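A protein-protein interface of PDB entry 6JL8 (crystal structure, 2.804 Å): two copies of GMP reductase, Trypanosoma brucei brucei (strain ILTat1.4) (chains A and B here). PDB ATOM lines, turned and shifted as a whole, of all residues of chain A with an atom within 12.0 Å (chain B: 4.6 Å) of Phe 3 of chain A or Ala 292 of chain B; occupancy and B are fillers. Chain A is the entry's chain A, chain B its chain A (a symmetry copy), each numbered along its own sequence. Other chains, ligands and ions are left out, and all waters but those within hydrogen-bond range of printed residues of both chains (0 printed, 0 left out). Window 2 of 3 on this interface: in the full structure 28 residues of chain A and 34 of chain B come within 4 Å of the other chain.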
ATOM      1  N   PHE A   3      17.806  -1.119  21.975  1.00  0.00           N
ATOM      2  CA  PHE A   3      16.734  -1.954  21.418  1.00  0.00           C
ATOM      3  C   PHE A   3      16.516  -3.230  22.263  1.00  0.00           C
ATOM      4  O   PHE A   3      16.711  -4.351  21.792  1.00  0.00           O
ATOM      5  CB  PHE A   3      17.037  -2.277  19.927  1.00  0.00           C
ATOM      6  CG  PHE A   3      16.930  -1.059  19.037  1.00  0.00           C
ATOM      7  CD1 PHE A   3      15.725  -0.752  18.388  1.00  0.00           C
ATOM      8  CD2 PHE A   3      17.994  -0.153  18.938  1.00  0.00           C
ATOM      9  CE1 PHE A   3      15.591   0.431  17.611  1.00  0.00           C
ATOM     10  CE2 PHE A   3      17.879   1.038  18.165  1.00  0.00           C
ATOM     11  CZ  PHE A   3      16.675   1.326  17.498  1.00  0.00           C
ATOM     12  N   ASN A   4      16.080  -3.037  23.515  1.00  0.00           N
ATOM     13  CA  ASN A   4      16.048  -4.140  24.476  1.00  0.00           C
ATOM     14  C   ASN A   4      14.767  -4.951  24.368  1.00  0.00           C
ATOM     15  O   ASN A   4      14.810  -6.181  24.459  1.00  0.00           O
ATOM     16  CB  ASN A   4      16.210  -3.619  25.915  1.00  0.00           C
ATOM     17  CG  ASN A   4      15.322  -2.408  26.208  1.00  0.00           C
ATOM     18  OD1 ASN A   4      15.663  -1.279  25.848  1.00  0.00           O
ATOM     19  ND2 ASN A   4      14.172  -2.639  26.848  1.00  0.00           N
ATOM     20  N   GLU A   5      13.621  -4.282  24.194  1.00  0.00           N
ATOM     21  CA  GLU A   5      12.318  -4.939  24.075  1.00  0.00           C
ATOM     22  C   GLU A   5      12.362  -6.148  23.139  1.00  0.00           C
ATOM     23  O   GLU A   5      11.584  -7.094  23.280  1.00  0.00           O
ATOM     24  CB  GLU A   5      11.263  -3.948  23.563  1.00  0.00           C
ATOM     25  CG  GLU A   5      11.291  -2.543  24.212  1.00  0.00           C
ATOM     26  CD  GLU A   5      12.232  -1.553  23.510  1.00  0.00           C
ATOM     27  OE1 GLU A   5      12.103  -0.331  23.784  1.00  0.00           O
ATOM     28  OE2 GLU A   5      13.096  -1.998  22.704  1.00  0.00           O
ATOM     29  N   SER A   6      13.268  -6.117  22.176  1.00  0.00           N
ATOM     30  CA  SER A   6      13.436  -7.172  21.199  1.00  0.00           C
ATOM     31  C   SER A   6      14.445  -8.233  21.635  1.00  0.00           C
ATOM     32  O   SER A   6      14.660  -9.207  20.914  1.00  0.00           O
ATOM     33  CB  SER A   6      13.884  -6.547  19.885  1.00  0.00           C
ATOM     34  OG  SER A   6      13.263  -5.285  19.673  1.00  0.00           O
ATOM     35  N   ALA A   7      15.056  -8.095  22.798  1.00  0.00           N
ATOM     36  CA  ALA A   7      15.994  -9.101  23.259  1.00  0.00           C
ATOM     37  C   ALA A   7      15.354 -10.114  24.207  1.00  0.00           C
ATOM     38  O   ALA A   7      15.932 -11.181  24.446  1.00  0.00           O
ATOM     39  CB  ALA A   7      17.199  -8.418  23.923  1.00  0.00           C
ATOM     40  N   SER A   8      14.165  -9.827  24.727  1.00  0.00           N
ATOM     41  CA  SER A   8      13.485 -10.736  25.635  1.00  0.00           C
ATOM     42  C   SER A   8      12.403 -11.560  24.939  1.00  0.00           C
ATOM     43  O   SER A   8      11.543 -12.143  25.609  1.00  0.00           O
ATOM     44  CB  SER A   8      12.895  -9.945  26.796  1.00  0.00           C
ATOM     45  OG  SER A   8      12.136  -8.858  26.286  1.00  0.00           O
ATOM     46  N   ILE A   9      12.418 -11.610  23.612  1.00  0.00           N
ATOM     47  CA  ILE A   9      11.552 -12.520  22.874  1.00  0.00           C
ATOM     48  C   ILE A   9      12.248 -13.875  22.814  1.00  0.00           C
ATOM     49  O   ILE A   9      13.367 -13.976  22.311  1.00  0.00           O
ATOM     50  CB  ILE A   9      11.233 -11.985  21.471  1.00  0.00           C
ATOM     51  CG1 ILE A   9      10.248 -10.815  21.550  1.00  0.00           C
ATOM     52  CG2 ILE A   9      10.644 -13.076  20.640  1.00  0.00           C
ATOM     53  CD1 ILE A   9      10.299  -9.869  20.374  1.00  0.00           C
ATOM     54  N   PRO A  10      11.651 -14.936  23.325  1.00  0.00           N
ATOM     55  CA  PRO A  10      12.296 -16.243  23.223  1.00  0.00           C
ATOM     56  C   PRO A  10      12.293 -16.710  21.781  1.00  0.00           C
ATOM     57  O   PRO A  10      11.564 -16.195  20.933  1.00  0.00           O
ATOM     58  CB  PRO A  10      11.426 -17.136  24.099  1.00  0.00           C
ATOM     59  CG  PRO A  10      10.054 -16.534  23.942  1.00  0.00           C
ATOM     60  CD  PRO A  10      10.274 -15.035  23.843  1.00  0.00           C
ATOM     61  N   PRO B  10      23.034  -4.726  19.247  1.00  0.00           N
ATOM     62  CA  PRO B  10      21.754  -5.395  19.467  1.00  0.00           C
ATOM     63  C   PRO B  10      21.210  -5.916  18.152  1.00  0.00           C
ATOM     64  O   PRO B  10      21.645  -5.525  17.069  1.00  0.00           O
ATOM     65  CB  PRO B  10      20.872  -4.290  20.035  1.00  0.00           C
ATOM     66  CG  PRO B  10      21.403  -3.051  19.363  1.00  0.00           C
ATOM     67  CD  PRO B  10      22.903  -3.258  19.249  1.00  0.00           C
ATOM     68  N   ILE B 291      10.480   7.991  11.862  1.00  0.00           N
ATOM     69  CA  ILE B 291      11.415   7.750  12.944  1.00  0.00           C
ATOM     70  C   ILE B 291      11.582   6.241  13.127  1.00  0.00           C
ATOM     71  O   ILE B 291      11.004   5.447  12.380  1.00  0.00           O
ATOM     72  CB  ILE B 291      10.985   8.453  14.247  1.00  0.00           C
ATOM     73  CG1 ILE B 291       9.563   8.101  14.606  1.00  0.00           C
ATOM     74  CG2 ILE B 291      11.043   9.936  14.062  1.00  0.00           C
ATOM     75  CD1 ILE B 291       9.252   8.519  15.962  1.00  0.00           C
ATOM     76  N   ALA B 292      12.413   5.852  14.116  1.00  0.00           N
ATOM     77  CA  ALA B 292      12.732   4.440  14.311  1.00  0.00           C
ATOM     78  C   ALA B 292      13.519   4.178  15.592  1.00  0.00           C
ATOM     79  O   ALA B 292      13.964   3.052  15.825  1.00  0.00           O
ATOM     80  CB  ALA B 292      13.507   3.900  13.102  1.00  0.00           C
ATOM     81  N   SER B 293      13.721   5.200  16.415  1.00  0.00           N
ATOM     82  CA  SER B 293      14.277   5.040  17.754  1.00  0.00           C
ATOM     83  C   SER B 293      13.292   5.587  18.769  1.00  0.00           C
ATOM     84  O   SER B 293      12.445   6.424  18.449  1.00  0.00           O
ATOM     85  CB  SER B 293      15.621   5.774  17.930  1.00  0.00           C
ATOM     86  OG  SER B 293      15.579   7.086  17.369  1.00  0.00           O
ATOM     87  N   ALA B 294      13.441   5.139  20.017  1.00  0.00           N
ATOM     88  CA  ALA B 294      12.796   5.826  21.135  1.00  0.00           C
ATOM     89  C   ALA B 294      13.162   7.315  21.159  1.00  0.00           C
ATOM     90  O   ALA B 294      12.287   8.187  21.294  1.00  0.00           O
ATOM     91  CB  ALA B 294      13.187   5.149  22.437  1.00  0.00           C
ATOM     92  N   ALA B 296      14.008   9.441  18.845  1.00  0.00           N
ATOM     93  CA  ALA B 296      13.331  10.247  17.826  1.00  0.00           C
ATOM     94  C   ALA B 296      11.868  10.497  18.180  1.00  0.00           C
ATOM     95  O   ALA B 296      11.379  11.631  18.061  1.00  0.00           O
ATOM     96  CB  ALA B 296      13.434   9.548  16.489  1.00  0.00           C
ATOM     97  N   VAL B 312      12.202   3.878   9.274  1.00  0.00           N
ATOM     98  CA  VAL B 312      13.308   4.301   8.423  1.00  0.00           C
ATOM     99  C   VAL B 312      13.792   3.044   7.725  1.00  0.00           C
ATOM    100  O   VAL B 312      14.485   2.231   8.351  1.00  0.00           O
ATOM    101  CB  VAL B 312      14.437   4.937   9.234  1.00  0.00           C
ATOM    102  CG1 VAL B 312      15.728   5.002   8.421  1.00  0.00           C
ATOM    103  CG2 VAL B 312      14.049   6.325   9.728  1.00  0.00           C
ATOM    104  N   VAL B 328      16.230   0.515  10.720  1.00  0.00           N
ATOM    105  CA  VAL B 328      16.037  -0.335  11.884  1.00  0.00           C
ATOM    106  C   VAL B 328      14.983  -1.355  11.480  1.00  0.00           C
ATOM    107  O   VAL B 328      13.963  -0.965  10.908  1.00  0.00           O
ATOM    108  CB  VAL B 328      15.601   0.468  13.129  1.00  0.00           C
ATOM    109  CG1 VAL B 328      15.331  -0.467  14.292  1.00  0.00           C
ATOM    110  CG2 VAL B 328      16.636   1.498  13.531  1.00  0.00           C
ATOM    111  N   SER B 332      11.190  -4.106  15.663  1.00  0.00           N
ATOM    112  CA  SER B 332      11.980  -3.441  16.694  1.00  0.00           C
ATOM    113  C   SER B 332      11.713  -1.950  16.719  1.00  0.00           C
ATOM    114  O   SER B 332      11.707  -1.328  17.793  1.00  0.00           O
ATOM    115  CB  SER B 332      13.480  -3.698  16.431  1.00  0.00           C
ATOM    116  OG  SER B 332      13.872  -4.985  16.874  1.00  0.00           O
ATOM    117  N   ALA B 333      11.618  -1.353  15.528  1.00  0.00           N
ATOM    118  CA  ALA B 333      11.323   0.069  15.444  1.00  0.00           C
ATOM    119  C   ALA B 333      10.023   0.391  16.175  1.00  0.00           C
ATOM    120  O   ALA B 333       9.958   1.330  16.977  1.00  0.00           O
ATOM    121  CB  ALA B 333      11.235   0.491  13.986  1.00  0.00           C
ATOM    122  N   ALA B 336      10.080   0.022  19.948  1.00  0.00           N
ATOM    123  CA  ALA B 336      10.860   1.047  20.629  1.00  0.00           C
ATOM    124  C   ALA B 336      10.096   2.359  20.728  1.00  0.00           C
ATOM    125  O   ALA B 336      10.080   3.015  21.781  1.00  0.00           O
ATOM    126  CB  ALA B 336      12.165   1.270  19.883  1.00  0.00           C
ATOM    127  N   CYS B 337       9.496   2.777  19.618  1.00  0.00           N
ATOM    128  CA  CYS B 337       8.879   4.090  19.529  1.00  0.00           C
ATOM    129  C   CYS B 337       7.567   4.139  20.302  1.00  0.00           C
ATOM    130  O   CYS B 337       7.205   5.175  20.860  1.00  0.00           O
ATOM    131  CB  CYS B 337       8.616   4.421  18.066  1.00  0.00           C
ATOM    132  SG  CYS B 337      10.070   4.602  17.056  1.00  0.00           S
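Among the printed residues, merely in contact across the chains: Phe 3 of chain A with Ala 292 of chain B (3.6 Å), Phe 3 of chain A with Val 328 of chain B (3.4 Å) and Glu 5 of chain A with Ala 336 of chain B (3.7 Å).
Position printed for both chains: 10. Of the 4 pairs that touch across the chains among the printed residues, none has its exchanged pair printed and touching as well.
OG of Ser 6 of chain A lies within hydrogen-bond range of OG of Ser 332 of chain B.
The backbone carbonyl oxygen (O) of Val 312 of chain B lies within hydrogen-bond range of the backbone NH (N) of Val 328 of chain B (3.4 Å).
Hydrophobic or aromatic side chains of chain A within 4 Å of the printed part of chain B: Phe 3. Of the 12 printed residues of chain B, 4 touch a printed residue of chain A. Hydrophobic or aromatic side chains of chain B within 4 Å of the printed part of chain A: Val 328. Among the printed residues, no Asp or Glu carboxylate lies within 4 Å of a Lys or Arg side-chain nitrogen of the other chain.
Asn 4 of chain A touches none of the printed residues of chain B. Of the printed residues of chain B, Glu 5 of chain A touches Ala 336. Printed residues of chain B within 4 Å of Ser 6 of chain A: Ser 332. Ser 8 of chain A touches none of the printed residues of chain B. No residue of chain A comes within 4 Å of Pro 10 of chain B. No residue of chain A comes within 4 Å of Ile 291 of chain B. Ala 292 of chain B touches one residue of chain A. No residue of chain A comes within 4 Å of Ser 293 of chain B. No residue of chain A comes within 4 Å of Val 312 of chain B. Ser 332 of chain B touches just one residue of chain A: Ser 6. No residue of chain A comes within 4 Å of Ala 333 of chain B. The nearest residue of chain B that does not touch Phe 3 of chain A is Ser 332 of chain B (4.1 Å). The nearest residue of chain A that does not touch Ala 292 of chain B is Glu 5 of chain A (8.6 Å).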
